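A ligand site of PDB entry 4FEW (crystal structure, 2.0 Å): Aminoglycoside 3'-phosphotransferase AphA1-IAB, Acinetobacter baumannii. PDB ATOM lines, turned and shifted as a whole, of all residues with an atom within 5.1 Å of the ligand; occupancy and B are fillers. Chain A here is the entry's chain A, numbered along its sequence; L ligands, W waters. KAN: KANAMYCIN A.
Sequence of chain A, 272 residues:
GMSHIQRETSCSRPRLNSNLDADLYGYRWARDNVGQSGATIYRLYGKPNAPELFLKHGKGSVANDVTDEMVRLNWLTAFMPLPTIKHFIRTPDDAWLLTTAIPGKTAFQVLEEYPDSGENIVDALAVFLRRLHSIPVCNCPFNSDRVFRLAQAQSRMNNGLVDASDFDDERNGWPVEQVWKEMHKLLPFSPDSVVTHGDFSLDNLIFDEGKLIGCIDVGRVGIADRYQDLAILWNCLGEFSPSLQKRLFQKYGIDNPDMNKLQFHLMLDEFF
N2 of the ligand is in salt-bridge range of OD2 of Asp 269 (3.9 Å). The side-chain carboxylate (OD1) of Asp 168 is in salt-bridge range of a nitrogen (N3) of the ligand. O of Gln 36 is in hydrogen-bond range of O8 of the ligand (2.8 Å). O of Asp 269 lies within hydrogen-bond range of N2 of the ligand (2.7 Å). An oxygen (O14) of the ligand is in hydrogen-bond range of the backbone carbonyl oxygen (O) of Asn 235 (3.4 Å). An oxygen (O8) of the ligand is in hydrogen-bond range of the guanidinium group (NH2) of Arg 220. An oxygen (O14) of the ligand lies close to the side-chain carboxylate of Glu 239 (3.4 Å). A nitrogen (N3) of the ligand lies close to the backbone NH (N) of Asp 168. OXT of Phe 272 lies within salt-bridge range of N2 of the ligand, at 2.8 Å. A nitrogen (N3) of the ligand is in hydrogen-bond range of the backbone carbonyl oxygen of Asp 166 (2.9 Å). The side-chain carboxylate of Asp 199 lies within hydrogen-bond range of an oxygen (O7) of the ligand (2.6 Å). The side-chain carboxylate of Glu 270 is in salt-bridge range of a nitrogen (N3) of the ligand (2.5 Å).
O of Phe 272 lies within salt-bridge range of NH1 of Arg 156 (3.8 Å). The backbone NH (N) of Asp 168 is in hydrogen-bond range of the side-chain carboxylate (OE2) of Glu 270 (2.8 Å). OE1 of Gln 36 sits close to OD2 of Asp 199 (3.1 Å). The guanidinium group (NH2) of Arg 220 is in salt-bridge range of the side-chain carboxylate (OD2) of Asp 199 (3.4 Å). O of Phe 272 is in salt-bridge range of NH1 of Arg 220, at 3.3 Å. The side-chain amide nitrogen of Asn 235 sits at hydrogen-bond distance from the side-chain carboxylate of Asp 168 (3.1 Å). O of Asp 199 sits at hydrogen-bond distance from ND2 of Asn 204, at 2.9 Å.
Residues that only touch the ligand: Phe 167 and Cys 236. Of the 20 residues printed, 12 come within 4 Å of the ligand. The nearest printed residue that does not touch the ligand is Asp 203 (4.7 Å).
Water W1 bridges an oxygen (O15) of the ligand (2.6 Å) and the side-chain sulfur of Cys 236 (3.7 Å). Water W4 bridges OG of Ser 201 and O6 of the ligand. Water W10 bridges the side-chain carboxylate (OD1) of Asp 269 (2.7 Å) and a nitrogen (N2) of the ligand (2.8 Å). Water W9 lies within hydrogen-bond range of N2 of the ligand, OD2 of Asp 166 and OXT of Phe 272. Water W5 bridges N1 of the ligand (2.8 Å) and OD2 of Asp 163 (3.0 Å). Water W6 lies within hydrogen-bond range of the side-chain carboxylate (OD1) of Asp 166 (3.0 Å) and an oxygen (O10) of the ligand (3.0 Å).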
ATOM      1  N   GLY A  35       7.735  -6.730 -34.729  1.00  0.00           N
ATOM      2  CA  GLY A  35       6.493  -7.460 -34.780  1.00  0.00           C
ATOM      3  C   GLY A  35       6.377  -8.383 -33.593  1.00  0.00           C
ATOM      4  O   GLY A  35       7.305  -8.476 -32.788  1.00  0.00           O
ATOM      5  N   GLN A  36       5.239  -9.071 -33.533  1.00  0.00           N
ATOM      6  CA  GLN A  36       4.790  -9.815 -32.357  1.00  0.00           C
ATOM      7  C   GLN A  36       5.878 -10.596 -31.635  1.00  0.00           C
ATOM      8  O   GLN A  36       6.090 -10.417 -30.431  1.00  0.00           O
ATOM      9  CB  GLN A  36       3.672 -10.780 -32.762  1.00  0.00           C
ATOM     10  CG  GLN A  36       2.910 -11.367 -31.603  1.00  0.00           C
ATOM     11  CD  GLN A  36       1.426 -11.451 -31.928  1.00  0.00           C
ATOM     12  OE1 GLN A  36       0.854 -10.515 -32.493  1.00  0.00           O
ATOM     13  NE2 GLN A  36       0.805 -12.576 -31.605  1.00  0.00           N
ATOM     14  N   SER A  37       6.551 -11.463 -32.375  1.00  0.00           N
ATOM     15  CA  SER A  37       7.560 -12.322 -31.772  1.00  0.00           C
ATOM     16  C   SER A  37       8.957 -12.056 -32.336  1.00  0.00           C
ATOM     17  O   SER A  37       9.863 -12.879 -32.199  1.00  0.00           O
ATOM     18  CB  SER A  37       7.153 -13.786 -31.914  1.00  0.00           C
ATOM     19  OG  SER A  37       5.868 -14.013 -31.346  1.00  0.00           O
ATOM     20  N   ARG A 156       9.681 -18.138 -20.935  1.00  0.00           N
ATOM     21  CA  ARG A 156      10.192 -16.845 -21.356  1.00  0.00           C
ATOM     22  C   ARG A 156      10.885 -16.126 -20.210  1.00  0.00           C
ATOM     23  O   ARG A 156      11.938 -15.520 -20.403  1.00  0.00           O
ATOM     24  CB  ARG A 156       9.085 -15.994 -21.973  1.00  0.00           C
ATOM     25  CG  ARG A 156       8.863 -16.329 -23.445  1.00  0.00           C
ATOM     26  CD  ARG A 156       7.831 -15.448 -24.111  1.00  0.00           C
ATOM     27  NE  ARG A 156       8.071 -14.022 -23.896  1.00  0.00           N
ATOM     28  CZ  ARG A 156       8.872 -13.266 -24.626  1.00  0.00           C
ATOM     29  NH1 ARG A 156       8.984 -11.971 -24.339  1.00  0.00           N
ATOM     30  NH2 ARG A 156       9.548 -13.780 -25.646  1.00  0.00           N
ATOM     31  N   ASP A 163      10.547  -8.591 -21.431  1.00  0.00           N
ATOM     32  CA  ASP A 163      10.927  -7.175 -21.511  1.00  0.00           C
ATOM     33  C   ASP A 163      10.456  -6.416 -20.273  1.00  0.00           C
ATOM     34  O   ASP A 163       9.355  -5.853 -20.246  1.00  0.00           O
ATOM     35  CB  ASP A 163      10.365  -6.524 -22.771  1.00  0.00           C
ATOM     36  CG  ASP A 163      10.882  -5.122 -22.980  1.00  0.00           C
ATOM     37  OD1 ASP A 163      11.588  -4.586 -22.096  1.00  0.00           O
ATOM     38  OD2 ASP A 163      10.570  -4.535 -24.046  1.00  0.00           O
ATOM     39  N   ASP A 166       9.060  -2.861 -20.263  1.00  0.00           N
ATOM     40  CA  ASP A 166       7.827  -2.575 -20.997  1.00  0.00           C
ATOM     41  C   ASP A 166       6.596  -2.922 -20.157  1.00  0.00           C
ATOM     42  O   ASP A 166       5.513  -3.041 -20.693  1.00  0.00           O
ATOM     43  CB  ASP A 166       7.808  -3.316 -22.348  1.00  0.00           C
ATOM     44  CG  ASP A 166       6.727  -2.786 -23.313  1.00  0.00           C
ATOM     45  OD1 ASP A 166       6.440  -1.573 -23.303  1.00  0.00           O
ATOM     46  OD2 ASP A 166       6.161  -3.593 -24.092  1.00  0.00           O
ATOM     47  N   PHE A 167       6.779  -3.083 -18.849  1.00  0.00           N
ATOM     48  CA  PHE A 167       5.644  -3.391 -17.991  1.00  0.00           C
ATOM     49  C   PHE A 167       4.663  -2.223 -17.944  1.00  0.00           C
ATOM     50  O   PHE A 167       5.039  -1.077 -18.231  1.00  0.00           O
ATOM     51  CB  PHE A 167       6.092  -3.745 -16.573  1.00  0.00           C
ATOM     52  CG  PHE A 167       6.824  -5.065 -16.462  1.00  0.00           C
ATOM     53  CD1 PHE A 167       6.720  -6.012 -17.465  1.00  0.00           C
ATOM     54  CD2 PHE A 167       7.596  -5.359 -15.352  1.00  0.00           C
ATOM     55  CE1 PHE A 167       7.393  -7.229 -17.374  1.00  0.00           C
ATOM     56  CE2 PHE A 167       8.267  -6.568 -15.249  1.00  0.00           C
ATOM     57  CZ  PHE A 167       8.169  -7.504 -16.258  1.00  0.00           C
ATOM     58  N   ASP A 168       3.413  -2.513 -17.595  1.00  0.00           N
ATOM     59  CA  ASP A 168       2.429  -1.454 -17.379  1.00  0.00           C
ATOM     60  C   ASP A 168       2.839  -0.581 -16.191  1.00  0.00           C
ATOM     61  O   ASP A 168       3.621  -1.004 -15.345  1.00  0.00           O
ATOM     62  CB  ASP A 168       1.029  -2.037 -17.118  1.00  0.00           C
ATOM     63  CG  ASP A 168       0.459  -2.784 -18.336  1.00  0.00           C
ATOM     64  OD1 ASP A 168       0.684  -2.358 -19.495  1.00  0.00           O
ATOM     65  OD2 ASP A 168      -0.241  -3.799 -18.119  1.00  0.00           O
ATOM     66  N   ASP A 169       2.296   0.630 -16.133  1.00  0.00           N
ATOM     67  CA  ASP A 169       2.711   1.606 -15.125  1.00  0.00           C
ATOM     68  C   ASP A 169       2.626   1.086 -13.695  1.00  0.00           C
ATOM     69  O   ASP A 169       3.508   1.349 -12.879  1.00  0.00           O
ATOM     70  CB  ASP A 169       1.915   2.913 -15.257  1.00  0.00           C
ATOM     71  CG  ASP A 169       2.268   3.670 -16.520  1.00  0.00           C
ATOM     72  OD1 ASP A 169       3.420   3.538 -16.992  1.00  0.00           O
ATOM     73  OD2 ASP A 169       1.386   4.395 -17.044  1.00  0.00           O
ATOM     74  N   ASP A 199      -3.878 -11.423 -29.057  1.00  0.00           N
ATOM     75  CA  ASP A 199      -3.195 -10.124 -28.950  1.00  0.00           C
ATOM     76  C   ASP A 199      -4.107  -9.001 -29.471  1.00  0.00           C
ATOM     77  O   ASP A 199      -3.765  -8.284 -30.434  1.00  0.00           O
ATOM     78  CB  ASP A 199      -1.900 -10.128 -29.757  1.00  0.00           C
ATOM     79  CG  ASP A 199      -0.948  -8.998 -29.366  1.00  0.00           C
ATOM     80  OD1 ASP A 199      -1.347  -8.150 -28.536  1.00  0.00           O
ATOM     81  OD2 ASP A 199       0.183  -8.951 -29.893  1.00  0.00           O
ATOM     82  N   SER A 201      -5.016  -5.996 -29.604  1.00  0.00           N
ATOM     83  CA  SER A 201      -4.620  -4.623 -29.315  1.00  0.00           C
ATOM     84  C   SER A 201      -5.166  -3.697 -30.395  1.00  0.00           C
ATOM     85  O   SER A 201      -5.690  -4.159 -31.416  1.00  0.00           O
ATOM     86  CB  SER A 201      -3.097  -4.494 -29.299  1.00  0.00           C
ATOM     87  OG  SER A 201      -2.600  -4.490 -30.632  1.00  0.00           O
ATOM     88  N   ASP A 203      -3.442  -2.048 -32.322  1.00  0.00           N
ATOM     89  CA  ASP A 203      -2.545  -2.162 -33.457  1.00  0.00           C
ATOM     90  C   ASP A 203      -2.996  -3.245 -34.434  1.00  0.00           C
ATOM     91  O   ASP A 203      -2.585  -3.260 -35.598  1.00  0.00           O
ATOM     92  CB  ASP A 203      -1.120  -2.493 -33.011  1.00  0.00           C
ATOM     93  CG  ASP A 203      -0.455  -1.357 -32.271  1.00  0.00           C
ATOM     94  OD1 ASP A 203      -0.694  -0.179 -32.627  1.00  0.00           O
ATOM     95  OD2 ASP A 203       0.317  -1.656 -31.330  1.00  0.00           O
ATOM     96  N   ASN A 204      -3.826  -4.167 -33.960  1.00  0.00           N
ATOM     97  CA  ASN A 204      -4.099  -5.393 -34.713  1.00  0.00           C
ATOM     98  C   ASN A 204      -5.484  -5.494 -35.352  1.00  0.00           C
ATOM     99  O   ASN A 204      -5.893  -6.564 -35.838  1.00  0.00           O
ATOM    100  CB  ASN A 204      -3.823  -6.599 -33.831  1.00  0.00           C
ATOM    101  CG  ASN A 204      -2.362  -6.789 -33.611  1.00  0.00           C
ATOM    102  OD1 ASN A 204      -1.563  -6.366 -34.437  1.00  0.00           O
ATOM    103  ND2 ASN A 204      -1.972  -7.400 -32.479  1.00  0.00           N
ATOM    104  N   ARG A 220      -1.251 -15.965 -31.804  1.00  0.00           N
ATOM    105  CA  ARG A 220      -1.614 -16.462 -30.476  1.00  0.00           C
ATOM    106  C   ARG A 220      -3.078 -16.926 -30.403  1.00  0.00           C
ATOM    107  O   ARG A 220      -3.611 -17.180 -29.322  1.00  0.00           O
ATOM    108  CB  ARG A 220      -1.322 -15.389 -29.418  1.00  0.00           C
ATOM    109  CG  ARG A 220       0.174 -15.063 -29.289  1.00  0.00           C
ATOM    110  CD  ARG A 220       0.517 -13.887 -28.334  1.00  0.00           C
ATOM    111  NE  ARG A 220       1.973 -13.670 -28.277  1.00  0.00           N
ATOM    112  CZ  ARG A 220       2.570 -12.470 -28.206  1.00  0.00           C
ATOM    113  NH1 ARG A 220       3.897 -12.400 -28.168  1.00  0.00           N
ATOM    114  NH2 ARG A 220       1.867 -11.343 -28.182  1.00  0.00           N
ATOM    115  N   ASN A 235      -6.704  -2.411 -21.800  1.00  0.00           N
ATOM    116  CA  ASN A 235      -5.422  -1.769 -21.501  1.00  0.00           C
ATOM    117  C   ASN A 235      -5.060  -0.715 -22.549  1.00  0.00           C
ATOM    118  O   ASN A 235      -4.670   0.390 -22.210  1.00  0.00           O
ATOM    119  CB  ASN A 235      -4.310  -2.820 -21.387  1.00  0.00           C
ATOM    120  CG  ASN A 235      -3.072  -2.299 -20.661  1.00  0.00           C
ATOM    121  OD1 ASN A 235      -3.161  -1.450 -19.765  1.00  0.00           O
ATOM    122  ND2 ASN A 235      -1.925  -2.807 -21.035  1.00  0.00           N
ATOM    123  N   CYS A 236      -5.204  -1.057 -23.829  1.00  0.00           N
ATOM    124  CA  CYS A 236      -4.868  -0.091 -24.883  1.00  0.00           C
ATOM    125  C   CYS A 236      -5.732   1.147 -24.791  1.00  0.00           C
ATOM    126  O   CYS A 236      -5.237   2.263 -24.950  1.00  0.00           O
ATOM    127  CB  CYS A 236      -5.040  -0.701 -26.281  1.00  0.00           C
ATOM    128  SG  CYS A 236      -3.857  -1.997 -26.705  1.00  0.00           S
ATOM    129  N   GLU A 239      -4.950   4.247 -22.600  1.00  0.00           N
ATOM    130  CA  GLU A 239      -4.066   5.344 -22.984  1.00  0.00           C
ATOM    131  C   GLU A 239      -4.912   6.545 -23.382  1.00  0.00           C
ATOM    132  O   GLU A 239      -4.414   7.670 -23.459  1.00  0.00           O
ATOM    133  CB  GLU A 239      -3.195   4.998 -24.184  1.00  0.00           C
ATOM    134  CG  GLU A 239      -2.438   3.695 -24.148  1.00  0.00           C
ATOM    135  CD  GLU A 239      -1.947   3.301 -25.534  1.00  0.00           C
ATOM    136  OE1 GLU A 239      -0.918   3.866 -25.980  1.00  0.00           O
ATOM    137  OE2 GLU A 239      -2.610   2.441 -26.200  1.00  0.00           O
ATOM    138  N   ASP A 269       0.225 -10.838 -19.900  1.00  0.00           N
ATOM    139  CA  ASP A 269       0.754 -10.291 -21.153  1.00  0.00           C
ATOM    140  C   ASP A 269       2.086  -9.556 -20.959  1.00  0.00           C
ATOM    141  O   ASP A 269       2.773  -9.224 -21.942  1.00  0.00           O
ATOM    142  CB  ASP A 269      -0.257  -9.340 -21.819  1.00  0.00           C
ATOM    143  CG  ASP A 269       0.061  -9.090 -23.291  1.00  0.00           C
ATOM    144  OD1 ASP A 269       0.363 -10.065 -24.010  1.00  0.00           O
ATOM    145  OD2 ASP A 269       0.010  -7.918 -23.727  1.00  0.00           O
ATOM    146  N   GLU A 270       2.429  -9.282 -19.698  1.00  0.00           N
ATOM    147  CA  GLU A 270       3.702  -8.643 -19.381  1.00  0.00           C
ATOM    148  C   GLU A 270       4.843  -9.564 -19.790  1.00  0.00           C
ATOM    149  O   GLU A 270       5.935  -9.122 -20.073  1.00  0.00           O
ATOM    150  CB  GLU A 270       3.818  -8.324 -17.883  1.00  0.00           C
ATOM    151  CG  GLU A 270       2.741  -7.397 -17.321  1.00  0.00           C
ATOM    152  CD  GLU A 270       2.931  -5.941 -17.705  1.00  0.00           C
ATOM    153  OE1 GLU A 270       3.287  -5.669 -18.865  1.00  0.00           O
ATOM    154  OE2 GLU A 270       2.713  -5.069 -16.832  1.00  0.00           O
ATOM    155  N   PHE A 272       5.058 -11.437 -22.457  1.00  0.00           N
ATOM    156  CA  PHE A 272       5.141 -11.721 -23.889  1.00  0.00           C
ATOM    157  C   PHE A 272       5.576 -10.555 -24.749  1.00  0.00           C
ATOM    158  O   PHE A 272       5.733 -10.715 -25.957  1.00  0.00           O
ATOM    159  CB  PHE A 272       3.817 -12.306 -24.399  1.00  0.00           C
ATOM    160  CG  PHE A 272       3.441 -13.592 -23.724  1.00  0.00           C
ATOM    161  CD1 PHE A 272       3.904 -14.801 -24.221  1.00  0.00           C
ATOM    162  CD2 PHE A 272       2.679 -13.596 -22.570  1.00  0.00           C
ATOM    163  CE1 PHE A 272       3.588 -15.992 -23.590  1.00  0.00           C
ATOM    164  CE2 PHE A 272       2.354 -14.784 -21.943  1.00  0.00           C
ATOM    165  CZ  PHE A 272       2.819 -15.983 -22.437  1.00  0.00           C
ATOM    166  OXT PHE A 272       5.794  -9.430 -24.275  1.00  0.00           O
HETATM  167  C1  KAN L   1       3.731  -5.313 -26.977  1.00  0.00           C
HETATM  168  C2  KAN L   1       2.959  -5.616 -28.263  1.00  0.00           C
HETATM  169  C3  KAN L   1       2.846  -7.114 -28.544  1.00  0.00           C
HETATM  170  C4  KAN L   1       4.232  -7.680 -28.662  1.00  0.00           C
HETATM  171  C5  KAN L   1       4.957  -7.440 -27.342  1.00  0.00           C
HETATM  172  C6  KAN L   1       6.357  -8.031 -27.458  1.00  0.00           C
HETATM  173  C7  KAN L   1       2.370  -4.550 -21.904  1.00  0.00           C
HETATM  174  C8  KAN L   1       2.643  -3.495 -22.927  1.00  0.00           C
HETATM  175  C9  KAN L   1       2.367  -4.124 -24.332  1.00  0.00           C
HETATM  176  C10 KAN L   1       3.264  -5.349 -24.607  1.00  0.00           C
HETATM  177  C11 KAN L   1       2.924  -6.407 -23.561  1.00  0.00           C
HETATM  178  C12 KAN L   1       3.196  -5.808 -22.197  1.00  0.00           C
HETATM  179  C13 KAN L   1       2.309  -1.067 -23.132  1.00  0.00           C
HETATM  180  C14 KAN L   1       1.803   0.014 -22.186  1.00  0.00           C
HETATM  181  C15 KAN L   1       0.279   0.044 -22.129  1.00  0.00           C
HETATM  182  C16 KAN L   1      -0.194   0.360 -23.544  1.00  0.00           C
HETATM  183  C17 KAN L   1       0.313  -0.728 -24.468  1.00  0.00           C
HETATM  184  C18 KAN L   1      -0.252  -0.578 -25.899  1.00  0.00           C
HETATM  185  N1  KAN L   1       7.045  -7.824 -26.184  1.00  0.00           N
HETATM  186  N2  KAN L   1       3.855  -7.528 -23.779  1.00  0.00           N
HETATM  187  N3  KAN L   1       2.768  -3.959 -20.606  1.00  0.00           N
HETATM  188  N4  KAN L   1      -0.177   1.028 -21.134  1.00  0.00           N
HETATM  189  O5  KAN L   1       5.010  -5.969 -27.072  1.00  0.00           O
HETATM  190  O6  KAN L   1       1.642  -5.053 -28.147  1.00  0.00           O
HETATM  191  O7  KAN L   1       2.161  -7.342 -29.787  1.00  0.00           O
HETATM  192  O8  KAN L   1       4.127  -9.078 -28.965  1.00  0.00           O
HETATM  193  O9  KAN L   1       3.000  -5.920 -25.885  1.00  0.00           O
HETATM  194  O10 KAN L   1       2.532  -3.129 -25.359  1.00  0.00           O
HETATM  195  O11 KAN L   1       1.845  -2.355 -22.576  1.00  0.00           O
HETATM  196  O12 KAN L   1       1.782  -0.790 -24.444  1.00  0.00           O
HETATM  197  O13 KAN L   1       2.366  -0.270 -20.914  1.00  0.00           O
HETATM  198  O14 KAN L   1      -1.598   0.440 -23.601  1.00  0.00           O
HETATM  199  O15 KAN L   1       0.130  -1.733 -26.681  1.00  0.00           O
HETATM  200  O   HOH W   1      -0.875  -4.087 -26.146  1.00  0.00           O
HETATM  201  O   HOH W   2       0.282   3.613 -21.780  1.00  0.00           O
HETATM  202  O   HOH W   3      -1.136  -1.414 -28.944  1.00  0.00           O
HETATM  203  O   HOH W   4      -0.058  -5.133 -30.327  1.00  0.00           O
HETATM  204  O   HOH W   5       8.527  -5.395 -26.059  1.00  0.00           O
HETATM  205  O   HOH W   6       4.645  -0.941 -25.566  1.00  0.00           O
HETATM  206  O   HOH W   7      -3.189   1.844 -20.419  1.00  0.00           O
HETATM  207  O   HOH W   8       1.258  -5.621 -32.599  1.00  0.00           O
HETATM  208  O   HOH W   9       6.473  -6.463 -23.575  1.00  0.00           O
HETATM  209  O   HOH W  10       2.334  -9.004 -25.572  1.00  0.00           O
HETATM  210  O   HOH W  11       6.634  -3.348 -26.644  1.00  0.00           O
HETATM  211  O   HOH W  12       2.593  -2.318 -28.637  1.00  0.00           O
HETATM  212  O   HOH W  13       9.627  -9.181 -25.968  1.00  0.00           O
HETATM  213  O   HOH W  14       4.063   1.728 -19.415  1.00  0.00           O
HETATM  214  O   HOH W  15       5.370   0.210 -21.711  1.00  0.00           O
HETATM  215  O   HOH W  16      -0.095  -6.855 -26.310  1.00  0.00           O
